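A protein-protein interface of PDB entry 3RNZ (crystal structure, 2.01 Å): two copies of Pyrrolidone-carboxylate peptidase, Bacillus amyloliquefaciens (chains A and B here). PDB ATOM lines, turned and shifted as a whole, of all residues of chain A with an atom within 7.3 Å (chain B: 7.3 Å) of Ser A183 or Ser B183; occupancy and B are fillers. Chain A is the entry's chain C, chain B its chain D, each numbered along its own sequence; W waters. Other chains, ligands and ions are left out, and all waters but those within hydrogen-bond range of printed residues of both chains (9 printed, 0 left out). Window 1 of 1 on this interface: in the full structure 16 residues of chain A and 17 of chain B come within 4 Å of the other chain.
Among the printed residues, merely in contact across the chains: Pro A132 with Thr B176 (3.5 Å), Thr A176 with Pro B132 (3.5 Å), His A188 with Ser B185 (3.8 Å), His A188 with Pro B173 (3.8 Å), Pro A173 with His B188 (3.9 Å), Pro A173 with Pro B132 (3.9 Å) and Ser A185 with His B188 (3.9 Å).
Water W5 lies within hydrogen-bond range of the side-chain hydroxyl of Ser A183, the backbone carbonyl oxygen of Ala A181, the side-chain hydroxyl of Thr A176 and the backbone carbonyl oxygen of Met B76.
Water W4 lies within hydrogen-bond range of the backbone carbonyl oxygen (O) of Ser B183 (2.7 Å) and the backbone NH (N) of Ser A183 (3.1 Å).
Water W9 lies within hydrogen-bond range of the side-chain hydroxyl of Ser A183 (2.8 Å), the backbone NH of Leu A184 (3.4 Å) and the backbone carbonyl oxygen of Ser B183 (3.4 Å).
Water W8 lies within hydrogen-bond range of the backbone carbonyl oxygen of Thr A176 (3.0 Å), the backbone NH of Ala A181 (3.0 Å) and the backbone carbonyl oxygen of Met B76 (3.4 Å).
Water W1 bridges the backbone carbonyl oxygen of Thr B176 (3.3 Å) and the side-chain amide nitrogen of Gln A77 (3.4 Å).
Of the 19 printed residues of chain A, 9 touch a printed residue of chain B.
Hydrophobic or aromatic side chains of chain A within 4 Å of the printed part of chain B: Met A76, Pro A132, Pro A173, Pro A182 and His A188.
Met A76 touches Ala B181, and with the chains exchanged Ala A181 touches Met B76.
Pro A132 touches Thr B176, and with the chains exchanged Thr A176 touches Pro B132.
Pro A173 touches Pro B132, but with the chains exchanged Pro A132 does not touch Pro B173 (4.04 Å).
Ser A185 touches His B188, and with the chains exchanged His A188 touches Ser B185.
Positions printed for both chains: 74, 75, 76, 77, 132, 170, 171, 172, 173, 174, 175, 176, 181, 182, 183, 184, 185, 188 and 189.
N of Ala A181 lies close to SD of Met B76 (3.4 Å).
The side-chain sulfur (SD) of Met A76 lies close to the backbone NH (N) of Ala B181 (3.7 Å).
The side-chain sulfur of Met B76 lies close to the backbone nitrogen of Pro A182 (3.7 Å).
The side-chain sulfur (SD) of Met A76 lies close to the backbone nitrogen (N) of Pro B182.
The backbone carbonyl oxygen (O) of Ser B183 lies close to the backbone carbonyl oxygen (O) of Ser A183.
The side-chain hydroxyl (OG) of Ser A185 is in hydrogen-bond range of the backbone NH (N) of His A188.
The side-chain hydroxyl (OG1) of Thr B176 lies within hydrogen-bond range of the backbone carbonyl oxygen (O) of Pro B173.
OG of Ser B185 sits at hydrogen-bond distance from N of His B188 (3.2 Å).
O of Pro A173 lies within hydrogen-bond range of OG1 of Thr A176 (2.6 Å).
Of chain B, only Ser B183 (3.5 Å) comes within 4 Å of Ser A183.
Of the printed residues of chain A, Ser B183 touches Ser A183 (3.5 Å).
Printed residues of chain B within 4 Å of Ser A185: His B188.
Of the printed residues of chain B, Pro A173 touches Pro B132 (3.9 Å) and His B188 (3.9 Å).
Of the printed residues of chain B, Pro A182 touches Met B76.
Of the printed residues of chain A, Ser B185 touches His A188 (3.8 Å).
Printed residues of chain B within 4 Å of Thr A176: Pro B132.
Tyr A171 touches none of the printed residues of chain B.
Gln A175 touches none of the printed residues of chain B.
The nearest residue of chain A that does not touch Ser B183 is Leu A184 (4.2 Å).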
ATOM      1  N   GLY A  74     -25.739 -30.912 -14.841  1.00  0.00           N
ATOM      2  CA  GLY A  74     -25.848 -29.552 -14.358  1.00  0.00           C
ATOM      3  C   GLY A  74     -24.482 -29.034 -13.913  1.00  0.00           C
ATOM      4  O   GLY A  74     -24.249 -27.816 -13.903  1.00  0.00           O
ATOM      5  N   ARG A  75     -23.559 -29.934 -13.532  1.00  0.00           N
ATOM      6  CA  ARG A  75     -22.248 -29.469 -13.116  1.00  0.00           C
ATOM      7  C   ARG A  75     -21.429 -29.112 -14.370  1.00  0.00           C
ATOM      8  O   ARG A  75     -21.769 -29.543 -15.450  1.00  0.00           O
ATOM      9  CB  ARG A  75     -21.532 -30.544 -12.310  1.00  0.00           C
ATOM     10  CG  ARG A  75     -22.239 -30.813 -10.949  1.00  0.00           C
ATOM     11  CD  ARG A  75     -21.385 -31.590  -9.936  1.00  0.00           C
ATOM     12  NE  ARG A  75     -22.142 -31.712  -8.662  1.00  0.00           N
ATOM     13  CZ  ARG A  75     -21.743 -32.465  -7.641  1.00  0.00           C
ATOM     14  NH1 ARG A  75     -20.601 -33.149  -7.748  1.00  0.00           N
ATOM     15  NH2 ARG A  75     -22.491 -32.550  -6.530  1.00  0.00           N
ATOM     16  N   MET A  76     -20.325 -28.389 -14.185  1.00  0.00           N
ATOM     17  CA  MET A  76     -19.511 -27.876 -15.289  1.00  0.00           C
ATOM     18  C   MET A  76     -18.063 -28.262 -15.183  1.00  0.00           C
ATOM     19  O   MET A  76     -17.274 -27.711 -15.891  1.00  0.00           O
ATOM     20  CB  MET A  76     -19.527 -26.344 -15.255  1.00  0.00           C
ATOM     21  CG  MET A  76     -20.885 -25.739 -15.362  1.00  0.00           C
ATOM     22  SD  MET A  76     -20.859 -24.023 -14.774  1.00  0.00           S
ATOM     23  CE  MET A  76     -22.487 -23.548 -15.505  1.00  0.00           C
ATOM     24  N   GLN A  77     -17.734 -29.170 -14.279  1.00  0.00           N
ATOM     25  CA  GLN A  77     -16.358 -29.596 -14.009  1.00  0.00           C
ATOM     26  C   GLN A  77     -16.365 -31.069 -13.627  1.00  0.00           C
ATOM     27  O   GLN A  77     -17.400 -31.586 -13.219  1.00  0.00           O
ATOM     28  CB  GLN A  77     -15.827 -28.858 -12.779  1.00  0.00           C
ATOM     29  CG  GLN A  77     -15.854 -27.343 -12.903  1.00  0.00           C
ATOM     30  CD  GLN A  77     -15.899 -26.648 -11.568  1.00  0.00           C
ATOM     31  OE1 GLN A  77     -16.814 -26.885 -10.771  1.00  0.00           O
ATOM     32  NE2 GLN A  77     -14.907 -25.762 -11.308  1.00  0.00           N
ATOM     33  N   PRO A 132     -11.614 -28.576 -16.830  1.00  0.00           N
ATOM     34  CA  PRO A 132     -12.052 -28.063 -15.522  1.00  0.00           C
ATOM     35  C   PRO A 132     -12.364 -29.163 -14.497  1.00  0.00           C
ATOM     36  O   PRO A 132     -12.949 -30.210 -14.830  1.00  0.00           O
ATOM     37  CB  PRO A 132     -13.276 -27.176 -15.872  1.00  0.00           C
ATOM     38  CG  PRO A 132     -13.874 -27.848 -17.046  1.00  0.00           C
ATOM     39  CD  PRO A 132     -12.631 -28.349 -17.877  1.00  0.00           C
ATOM     40  N   PRO A 170     -19.977 -34.307 -15.541  1.00  0.00           N
ATOM     41  CA  PRO A 170     -21.099 -33.552 -16.141  1.00  0.00           C
ATOM     42  C   PRO A 170     -21.793 -34.373 -17.227  1.00  0.00           C
ATOM     43  O   PRO A 170     -21.374 -35.485 -17.545  1.00  0.00           O
ATOM     44  CB  PRO A 170     -20.396 -32.391 -16.849  1.00  0.00           C
ATOM     45  CG  PRO A 170     -19.087 -32.211 -16.100  1.00  0.00           C
ATOM     46  CD  PRO A 170     -18.673 -33.668 -15.827  1.00  0.00           C
ATOM     47  N   TYR A 171     -22.863 -33.813 -17.787  1.00  0.00           N
ATOM     48  CA  TYR A 171     -23.509 -34.392 -18.964  1.00  0.00           C
ATOM     49  C   TYR A 171     -22.499 -34.276 -20.110  1.00  0.00           C
ATOM     50  O   TYR A 171     -21.567 -33.470 -20.026  1.00  0.00           O
ATOM     51  CB  TYR A 171     -24.655 -33.510 -19.446  1.00  0.00           C
ATOM     52  CG  TYR A 171     -25.876 -33.494 -18.596  1.00  0.00           C
ATOM     53  CD1 TYR A 171     -26.552 -34.686 -18.312  1.00  0.00           C
ATOM     54  CD2 TYR A 171     -26.443 -32.276 -18.180  1.00  0.00           C
ATOM     55  CE1 TYR A 171     -27.776 -34.689 -17.633  1.00  0.00           C
ATOM     56  CE2 TYR A 171     -27.694 -32.262 -17.509  1.00  0.00           C
ATOM     57  CZ  TYR A 171     -28.329 -33.464 -17.244  1.00  0.00           C
ATOM     58  OH  TYR A 171     -29.514 -33.470 -16.562  1.00  0.00           O
ATOM     59  N   ILE A 172     -22.710 -35.047 -21.178  1.00  0.00           N
ATOM     60  CA  ILE A 172     -21.922 -34.876 -22.388  1.00  0.00           C
ATOM     61  C   ILE A 172     -22.882 -34.037 -23.271  1.00  0.00           C
ATOM     62  O   ILE A 172     -24.082 -34.026 -23.045  1.00  0.00           O
ATOM     63  CB  ILE A 172     -21.529 -36.200 -23.070  1.00  0.00           C
ATOM     64  CG1 ILE A 172     -22.769 -37.057 -23.365  1.00  0.00           C
ATOM     65  CG2 ILE A 172     -20.443 -36.894 -22.208  1.00  0.00           C
ATOM     66  CD1 ILE A 172     -22.422 -38.376 -24.125  1.00  0.00           C
ATOM     67  N   PRO A 173     -22.360 -33.327 -24.276  1.00  0.00           N
ATOM     68  CA  PRO A 173     -23.174 -32.462 -25.153  1.00  0.00           C
ATOM     69  C   PRO A 173     -24.480 -33.027 -25.698  1.00  0.00           C
ATOM     70  O   PRO A 173     -25.493 -32.338 -25.677  1.00  0.00           O
ATOM     71  CB  PRO A 173     -22.220 -32.057 -26.288  1.00  0.00           C
ATOM     72  CG  PRO A 173     -20.835 -32.266 -25.736  1.00  0.00           C
ATOM     73  CD  PRO A 173     -20.957 -33.417 -24.715  1.00  0.00           C
ATOM     74  N   GLU A 174     -24.428 -34.264 -26.179  1.00  0.00           N
ATOM     75  CA  GLU A 174     -25.562 -34.991 -26.741  1.00  0.00           C
ATOM     76  C   GLU A 174     -26.745 -35.145 -25.797  1.00  0.00           C
ATOM     77  O   GLU A 174     -27.838 -35.498 -26.246  1.00  0.00           O
ATOM     78  CB  GLU A 174     -25.115 -36.412 -27.159  1.00  0.00           C
ATOM     79  CG  GLU A 174     -24.030 -36.480 -28.271  1.00  0.00           C
ATOM     80  CD  GLU A 174     -22.698 -35.728 -27.952  1.00  0.00           C
ATOM     81  OE1 GLU A 174     -22.063 -35.998 -26.878  1.00  0.00           O
ATOM     82  OE2 GLU A 174     -22.293 -34.861 -28.819  1.00  0.00           O
ATOM     83  N   GLN A 175     -26.523 -34.930 -24.497  1.00  0.00           N
ATOM     84  CA  GLN A 175     -27.596 -35.047 -23.494  1.00  0.00           C
ATOM     85  C   GLN A 175     -28.263 -33.692 -23.242  1.00  0.00           C
ATOM     86  O   GLN A 175     -29.179 -33.582 -22.439  1.00  0.00           O
ATOM     87  CB  GLN A 175     -27.022 -35.542 -22.136  1.00  0.00           C
ATOM     88  CG  GLN A 175     -26.599 -37.048 -22.172  1.00  0.00           C
ATOM     89  CD  GLN A 175     -25.992 -37.469 -20.823  1.00  0.00           C
ATOM     90  OE1 GLN A 175     -24.937 -37.003 -20.470  1.00  0.00           O
ATOM     91  NE2 GLN A 175     -26.687 -38.314 -20.065  1.00  0.00           N
ATOM     92  N   THR A 176     -27.778 -32.662 -23.908  1.00  0.00           N
ATOM     93  CA  THR A 176     -28.276 -31.302 -23.640  1.00  0.00           C
ATOM     94  C   THR A 176     -28.891 -30.622 -24.861  1.00  0.00           C
ATOM     95  O   THR A 176     -28.821 -29.385 -25.010  1.00  0.00           O
ATOM     96  CB  THR A 176     -27.085 -30.430 -23.123  1.00  0.00           C
ATOM     97  OG1 THR A 176     -26.106 -30.259 -24.177  1.00  0.00           O
ATOM     98  CG2 THR A 176     -26.347 -31.181 -21.977  1.00  0.00           C
ATOM     99  N   ALA A 181     -27.925 -27.009 -20.849  1.00  0.00           N
ATOM    100  CA  ALA A 181     -27.247 -27.356 -19.618  1.00  0.00           C
ATOM    101  C   ALA A 181     -25.783 -27.491 -19.973  1.00  0.00           C
ATOM    102  O   ALA A 181     -25.456 -27.741 -21.107  1.00  0.00           O
ATOM    103  CB  ALA A 181     -27.800 -28.707 -19.075  1.00  0.00           C
ATOM    104  N   PRO A 182     -24.889 -27.333 -18.987  1.00  0.00           N
ATOM    105  CA  PRO A 182     -23.438 -27.451 -19.205  1.00  0.00           C
ATOM    106  C   PRO A 182     -23.062 -28.891 -19.549  1.00  0.00           C
ATOM    107  O   PRO A 182     -23.743 -29.865 -19.157  1.00  0.00           O
ATOM    108  CB  PRO A 182     -22.839 -27.082 -17.838  1.00  0.00           C
ATOM    109  CG  PRO A 182     -23.921 -26.371 -17.109  1.00  0.00           C
ATOM    110  CD  PRO A 182     -25.205 -26.998 -17.587  1.00  0.00           C
ATOM    111  N   SER A 183     -21.986 -29.063 -20.282  1.00  0.00           N
ATOM    112  CA  SER A 183     -21.519 -30.414 -20.562  1.00  0.00           C
ATOM    113  C   SER A 183     -19.988 -30.374 -20.803  1.00  0.00           C
ATOM    114  O   SER A 183     -19.411 -29.287 -20.884  1.00  0.00           O
ATOM    115  CB  SER A 183     -22.219 -30.956 -21.790  1.00  0.00           C
ATOM    116  OG  SER A 183     -21.919 -30.164 -22.942  1.00  0.00           O
ATOM    117  N   LEU A 184     -19.353 -31.553 -20.895  1.00  0.00           N
ATOM    118  CA  LEU A 184     -17.923 -31.690 -21.261  1.00  0.00           C
ATOM    119  C   LEU A 184     -17.980 -32.845 -22.254  1.00  0.00           C
ATOM    120  O   LEU A 184     -18.776 -33.785 -22.083  1.00  0.00           O
ATOM    121  CB  LEU A 184     -17.011 -32.087 -20.089  1.00  0.00           C
ATOM    122  CG  LEU A 184     -16.573 -30.986 -19.128  1.00  0.00           C
ATOM    123  CD1 LEU A 184     -15.771 -31.613 -17.958  1.00  0.00           C
ATOM    124  CD2 LEU A 184     -15.701 -29.971 -19.873  1.00  0.00           C
ATOM    125  N   SER A 185     -17.127 -32.811 -23.275  1.00  0.00           N
ATOM    126  CA  SER A 185     -17.191 -33.841 -24.295  1.00  0.00           C
ATOM    127  C   SER A 185     -16.788 -35.184 -23.696  1.00  0.00           C
ATOM    128  O   SER A 185     -16.047 -35.229 -22.699  1.00  0.00           O
ATOM    129  CB  SER A 185     -16.220 -33.494 -25.467  1.00  0.00           C
ATOM    130  OG  SER A 185     -14.883 -33.651 -24.996  1.00  0.00           O
ATOM    131  N   HIS A 188     -13.071 -35.556 -23.415  1.00  0.00           N
ATOM    132  CA  HIS A 188     -12.426 -34.885 -22.269  1.00  0.00           C
ATOM    133  C   HIS A 188     -12.688 -35.595 -20.927  1.00  0.00           C
ATOM    134  O   HIS A 188     -11.786 -35.723 -20.070  1.00  0.00           O
ATOM    135  CB  HIS A 188     -12.866 -33.408 -22.158  1.00  0.00           C
ATOM    136  CG  HIS A 188     -12.379 -32.540 -23.285  1.00  0.00           C
ATOM    137  ND1 HIS A 188     -11.384 -32.934 -24.162  1.00  0.00           N
ATOM    138  CD2 HIS A 188     -12.720 -31.280 -23.647  1.00  0.00           C
ATOM    139  CE1 HIS A 188     -11.132 -31.950 -25.011  1.00  0.00           C
ATOM    140  NE2 HIS A 188     -11.931 -30.934 -24.718  1.00  0.00           N
ATOM    141  N   ILE A 189     -13.915 -36.060 -20.752  1.00  0.00           N
ATOM    142  CA  ILE A 189     -14.269 -36.769 -19.511  1.00  0.00           C
ATOM    143  C   ILE A 189     -13.428 -38.048 -19.440  1.00  0.00           C
ATOM    144  O   ILE A 189     -12.899 -38.393 -18.384  1.00  0.00           O
ATOM    145  CB  ILE A 189     -15.779 -37.147 -19.503  1.00  0.00           C
ATOM    146  CG1 ILE A 189     -16.619 -35.888 -19.264  1.00  0.00           C
ATOM    147  CG2 ILE A 189     -16.084 -38.188 -18.375  1.00  0.00           C
ATOM    148  CD1 ILE A 189     -18.122 -36.134 -19.462  1.00  0.00           C
ATOM    149  N   GLY B  74     -20.362 -18.033 -20.836  1.00  0.00           N
ATOM    150  CA  GLY B  74     -21.494 -18.269 -19.946  1.00  0.00           C
ATOM    151  C   GLY B  74     -22.588 -19.035 -20.667  1.00  0.00           C
ATOM    152  O   GLY B  74     -23.347 -19.730 -20.026  1.00  0.00           O
ATOM    153  N   ARG B  75     -22.659 -18.936 -21.999  1.00  0.00           N
ATOM    154  CA  ARG B  75     -23.695 -19.676 -22.724  1.00  0.00           C
ATOM    155  C   ARG B  75     -23.267 -21.151 -22.839  1.00  0.00           C
ATOM    156  O   ARG B  75     -22.082 -21.455 -22.737  1.00  0.00           O
ATOM    157  CB  ARG B  75     -23.911 -19.070 -24.106  1.00  0.00           C
ATOM    158  CG  ARG B  75     -24.427 -17.633 -23.992  1.00  0.00           C
ATOM    159  CD  ARG B  75     -25.105 -17.164 -25.279  1.00  0.00           C
ATOM    160  NE  ARG B  75     -25.550 -15.773 -25.107  1.00  0.00           N
ATOM    161  CZ  ARG B  75     -25.957 -15.003 -26.113  1.00  0.00           C
ATOM    162  NH1 ARG B  75     -25.968 -15.483 -27.336  1.00  0.00           N
ATOM    163  NH2 ARG B  75     -26.357 -13.747 -25.902  1.00  0.00           N
ATOM    164  N   MET B  76     -24.233 -22.035 -23.031  1.00  0.00           N
ATOM    165  CA  MET B  76     -23.948 -23.462 -23.099  1.00  0.00           C
ATOM    166  C   MET B  76     -24.376 -24.117 -24.389  1.00  0.00           C
ATOM    167  O   MET B  76     -24.445 -25.338 -24.455  1.00  0.00           O
ATOM    168  CB  MET B  76     -24.594 -24.191 -21.912  1.00  0.00           C
ATOM    169  CG  MET B  76     -25.957 -23.701 -21.522  1.00  0.00           C
ATOM    170  SD  MET B  76     -26.482 -24.097 -19.778  1.00  0.00           S
ATOM    171  CE  MET B  76     -25.617 -22.978 -18.905  1.00  0.00           C
ATOM    172  N   GLN B  77     -24.620 -23.301 -25.416  1.00  0.00           N
ATOM    173  CA  GLN B  77     -25.060 -23.797 -26.724  1.00  0.00           C
ATOM    174  C   GLN B  77     -24.431 -22.911 -27.798  1.00  0.00           C
ATOM    175  O   GLN B  77     -24.024 -21.783 -27.502  1.00  0.00           O
ATOM    176  CB  GLN B  77     -26.578 -23.596 -26.905  1.00  0.00           C
ATOM    177  CG  GLN B  77     -27.498 -24.291 -25.866  1.00  0.00           C
ATOM    178  CD  GLN B  77     -28.850 -23.619 -25.705  1.00  0.00           C
ATOM    179  OE1 GLN B  77     -28.938 -22.418 -25.417  1.00  0.00           O
ATOM    180  NE2 GLN B  77     -29.916 -24.391 -25.876  1.00  0.00           N
ATOM    181  N   PRO B 132     -25.405 -28.968 -28.858  1.00  0.00           N
ATOM    182  CA  PRO B 132     -26.468 -28.061 -28.389  1.00  0.00           C
ATOM    183  C   PRO B 132     -26.446 -26.695 -29.111  1.00  0.00           C
ATOM    184  O   PRO B 132     -25.391 -26.080 -29.273  1.00  0.00           O
ATOM    185  CB  PRO B 132     -26.193 -27.936 -26.892  1.00  0.00           C
ATOM    186  CG  PRO B 132     -24.712 -28.161 -26.766  1.00  0.00           C
ATOM    187  CD  PRO B 132     -24.431 -29.257 -27.784  1.00  0.00           C
ATOM    188  N   PRO B 170     -19.839 -20.606 -27.058  1.00  0.00           N
ATOM    189  CA  PRO B 170     -19.434 -20.634 -25.650  1.00  0.00           C
ATOM    190  C   PRO B 170     -17.916 -20.567 -25.465  1.00  0.00           C
ATOM    191  O   PRO B 170     -17.137 -20.592 -26.413  1.00  0.00           O
ATOM    192  CB  PRO B 170     -19.923 -22.009 -25.154  1.00  0.00           C
ATOM    193  CG  PRO B 170     -20.958 -22.431 -26.169  1.00  0.00           C
ATOM    194  CD  PRO B 170     -20.422 -21.886 -27.483  1.00  0.00           C
ATOM    195  N   TYR B 171     -17.524 -20.545 -24.205  1.00  0.00           N
ATOM    196  CA  TYR B 171     -16.119 -20.659 -23.846  1.00  0.00           C
ATOM    197  C   TYR B 171     -15.677 -22.068 -24.270  1.00  0.00           C
ATOM    198  O   TYR B 171     -16.527 -22.960 -24.481  1.00  0.00           O
ATOM    199  CB  TYR B 171     -15.970 -20.687 -22.344  1.00  0.00           C
ATOM    200  CG  TYR B 171     -16.049 -19.381 -21.647  1.00  0.00           C
ATOM    201  CD1 TYR B 171     -15.284 -18.289 -22.083  1.00  0.00           C
ATOM    202  CD2 TYR B 171     -16.797 -19.256 -20.482  1.00  0.00           C
ATOM    203  CE1 TYR B 171     -15.262 -17.109 -21.350  1.00  0.00           C
ATOM    204  CE2 TYR B 171     -16.789 -18.099 -19.753  1.00  0.00           C
ATOM    205  CZ  TYR B 171     -16.018 -17.029 -20.186  1.00  0.00           C
ATOM    206  OH  TYR B 171     -15.981 -15.910 -19.406  1.00  0.00           O
ATOM    207  N   ILE B 172     -14.369 -22.269 -24.421  1.00  0.00           N
ATOM    208  CA  ILE B 172     -13.865 -23.630 -24.621  1.00  0.00           C
ATOM    209  C   ILE B 172     -13.404 -23.987 -23.200  1.00  0.00           C
ATOM    210  O   ILE B 172     -13.134 -23.108 -22.405  1.00  0.00           O
ATOM    211  CB  ILE B 172     -12.725 -23.744 -25.680  1.00  0.00           C
ATOM    212  CG1 ILE B 172     -11.605 -22.741 -25.380  1.00  0.00           C
ATOM    213  CG2 ILE B 172     -13.344 -23.562 -27.081  1.00  0.00           C
ATOM    214  CD1 ILE B 172     -10.400 -22.814 -26.386  1.00  0.00           C
ATOM    215  N   PRO B 173     -13.305 -25.280 -22.863  1.00  0.00           N
ATOM    216  CA  PRO B 173     -12.914 -25.781 -21.537  1.00  0.00           C
ATOM    217  C   PRO B 173     -11.719 -25.111 -20.858  1.00  0.00           C
ATOM    218  O   PRO B 173     -11.763 -24.779 -19.676  1.00  0.00           O
ATOM    219  CB  PRO B 173     -12.651 -27.278 -21.770  1.00  0.00           C
ATOM    220  CG  PRO B 173     -13.419 -27.594 -23.026  1.00  0.00           C
ATOM    221  CD  PRO B 173     -13.361 -26.351 -23.866  1.00  0.00           C
ATOM    222  N   GLU B 174     -10.649 -24.917 -21.612  1.00  0.00           N
ATOM    223  CA  GLU B 174      -9.459 -24.345 -21.019  1.00  0.00           C
ATOM    224  C   GLU B 174      -9.641 -22.902 -20.554  1.00  0.00           C
ATOM    225  O   GLU B 174      -8.782 -22.374 -19.852  1.00  0.00           O
ATOM    226  CB  GLU B 174      -8.295 -24.503 -21.993  1.00  0.00           C
ATOM    227  CG  GLU B 174      -8.590 -23.902 -23.316  1.00  0.00           C
ATOM    228  CD  GLU B 174      -8.782 -24.975 -24.402  1.00  0.00           C
ATOM    229  OE1 GLU B 174      -9.803 -25.820 -24.331  1.00  0.00           O
ATOM    230  OE2 GLU B 174      -7.880 -24.910 -25.324  1.00  0.00           O
ATOM    231  N   GLN B 175     -10.743 -22.236 -20.946  1.00  0.00           N
ATOM    232  CA  GLN B 175     -10.982 -20.882 -20.436  1.00  0.00           C
ATOM    233  C   GLN B 175     -11.759 -20.975 -19.121  1.00  0.00           C
ATOM    234  O   GLN B 175     -12.044 -19.962 -18.502  1.00  0.00           O
ATOM    235  CB  GLN B 175     -11.847 -20.053 -21.405  1.00  0.00           C
ATOM    236  CG  GLN B 175     -11.162 -19.774 -22.749  1.00  0.00           C
ATOM    237  CD  GLN B 175     -12.092 -19.087 -23.731  1.00  0.00           C
ATOM    238  OE1 GLN B 175     -12.973 -19.726 -24.324  1.00  0.00           O
ATOM    239  NE2 GLN B 175     -11.883 -17.783 -23.930  1.00  0.00           N
ATOM    240  N   THR B 176     -12.118 -22.188 -18.683  1.00  0.00           N
ATOM    241  CA  THR B 176     -12.941 -22.276 -17.478  1.00  0.00           C
ATOM    242  C   THR B 176     -12.282 -23.027 -16.319  1.00  0.00           C
ATOM    243  O   THR B 176     -12.976 -23.691 -15.545  1.00  0.00           O
ATOM    244  CB  THR B 176     -14.285 -22.989 -17.827  1.00  0.00           C
ATOM    245  OG1 THR B 176     -14.026 -24.382 -18.131  1.00  0.00           O
ATOM    246  CG2 THR B 176     -14.935 -22.309 -19.061  1.00  0.00           C
ATOM    247  N   ALA B 181     -17.624 -22.401 -15.374  1.00  0.00           N
ATOM    248  CA  ALA B 181     -18.554 -21.864 -16.348  1.00  0.00           C
ATOM    249  C   ALA B 181     -18.724 -22.956 -17.389  1.00  0.00           C
ATOM    250  O   ALA B 181     -17.852 -23.816 -17.532  1.00  0.00           O
ATOM    251  CB  ALA B 181     -17.946 -20.581 -16.999  1.00  0.00           C
ATOM    252  N   PRO B 182     -19.856 -22.945 -18.125  1.00  0.00           N
ATOM    253  CA  PRO B 182     -20.124 -23.939 -19.162  1.00  0.00           C
ATOM    254  C   PRO B 182     -19.160 -23.728 -20.324  1.00  0.00           C
ATOM    255  O   PRO B 182     -18.670 -22.618 -20.527  1.00  0.00           O
ATOM    256  CB  PRO B 182     -21.548 -23.592 -19.624  1.00  0.00           C
ATOM    257  CG  PRO B 182     -22.130 -22.660 -18.549  1.00  0.00           C
ATOM    258  CD  PRO B 182     -20.922 -21.906 -18.084  1.00  0.00           C
ATOM    259  N   SER B 183     -18.908 -24.764 -21.110  1.00  0.00           N
ATOM    260  CA  SER B 183     -18.026 -24.612 -22.277  1.00  0.00           C
ATOM    261  C   SER B 183     -18.439 -25.686 -23.287  1.00  0.00           C
ATOM    262  O   SER B 183     -19.303 -26.516 -22.968  1.00  0.00           O
ATOM    263  CB  SER B 183     -16.535 -24.795 -21.849  1.00  0.00           C
ATOM    264  OG  SER B 183     -16.288 -26.084 -21.271  1.00  0.00           O
ATOM    265  N   LEU B 184     -17.883 -25.650 -24.503  1.00  0.00           N
ATOM    266  CA  LEU B 184     -18.094 -26.688 -25.527  1.00  0.00           C
ATOM    267  C   LEU B 184     -16.659 -26.877 -26.081  1.00  0.00           C
ATOM    268  O   LEU B 184     -15.887 -25.930 -26.135  1.00  0.00           O
ATOM    269  CB  LEU B 184     -18.999 -26.213 -26.680  1.00  0.00           C
ATOM    270  CG  LEU B 184     -20.520 -26.266 -26.539  1.00  0.00           C
ATOM    271  CD1 LEU B 184     -21.190 -25.846 -27.878  1.00  0.00           C
ATOM    272  CD2 LEU B 184     -20.938 -27.726 -26.151  1.00  0.00           C
ATOM    273  N   SER B 185     -16.299 -28.062 -26.522  1.00  0.00           N
ATOM    274  CA  SER B 185     -14.931 -28.214 -26.963  1.00  0.00           C
ATOM    275  C   SER B 185     -14.668 -27.474 -28.285  1.00  0.00           C
ATOM    276  O   SER B 185     -15.593 -27.252 -29.081  1.00  0.00           O
ATOM    277  CB  SER B 185     -14.591 -29.689 -27.126  1.00  0.00           C
ATOM    278  OG  SER B 185     -15.330 -30.189 -28.200  1.00  0.00           O
ATOM    279  N   HIS B 188     -15.888 -29.326 -31.187  1.00  0.00           N
ATOM    280  CA  HIS B 188     -17.331 -29.284 -31.421  1.00  0.00           C
ATOM    281  C   HIS B 188     -17.784 -27.937 -31.973  1.00  0.00           C
ATOM    282  O   HIS B 188     -18.709 -27.886 -32.799  1.00  0.00           O
ATOM    283  CB  HIS B 188     -18.154 -29.595 -30.157  1.00  0.00           C
ATOM    284  CG  HIS B 188     -18.122 -31.035 -29.742  1.00  0.00           C
ATOM    285  ND1 HIS B 188     -18.062 -32.077 -30.651  1.00  0.00           N
ATOM    286  CD2 HIS B 188     -18.241 -31.608 -28.524  1.00  0.00           C
ATOM    287  CE1 HIS B 188     -18.152 -33.227 -30.008  1.00  0.00           C
ATOM    288  NE2 HIS B 188     -18.264 -32.968 -28.718  1.00  0.00           N
ATOM    289  N   ILE B 189     -17.162 -26.867 -31.507  1.00  0.00           N
ATOM    290  CA  ILE B 189     -17.520 -25.503 -31.960  1.00  0.00           C
ATOM    291  C   ILE B 189     -17.141 -25.420 -33.437  1.00  0.00           C
ATOM    292  O   ILE B 189     -17.916 -24.934 -34.262  1.00  0.00           O
ATOM    293  CB  ILE B 189     -16.748 -24.474 -31.150  1.00  0.00           C
ATOM    294  CG1 ILE B 189     -17.308 -24.429 -29.714  1.00  0.00           C
ATOM    295  CG2 ILE B 189     -16.887 -23.067 -31.751  1.00  0.00           C
ATOM    296  CD1 ILE B 189     -16.493 -23.509 -28.811  1.00  0.00           C
HETATM  297  O   HOH W   1     -11.980 -25.492 -12.966  1.00  0.00           O
HETATM  298  O   HOH W   2     -16.968 -28.487 -22.799  1.00  0.00           O
HETATM  299  O   HOH W   3     -19.180 -27.195 -19.078  1.00  0.00           O
HETATM  300  O   HOH W   4     -21.843 -26.505 -21.999  1.00  0.00           O
HETATM  301  O   HOH W   5     -23.846 -28.321 -23.254  1.00  0.00           O
HETATM  302  O   HOH W   6     -15.823 -24.870 -15.281  1.00  0.00           O
HETATM  303  O   HOH W   7     -16.667 -25.921 -18.661  1.00  0.00           O
HETATM  304  O   HOH W   8     -27.179 -27.175 -23.801  1.00  0.00           O
HETATM  305  O   HOH W   9     -19.233 -29.835 -23.774  1.00  0.00           O
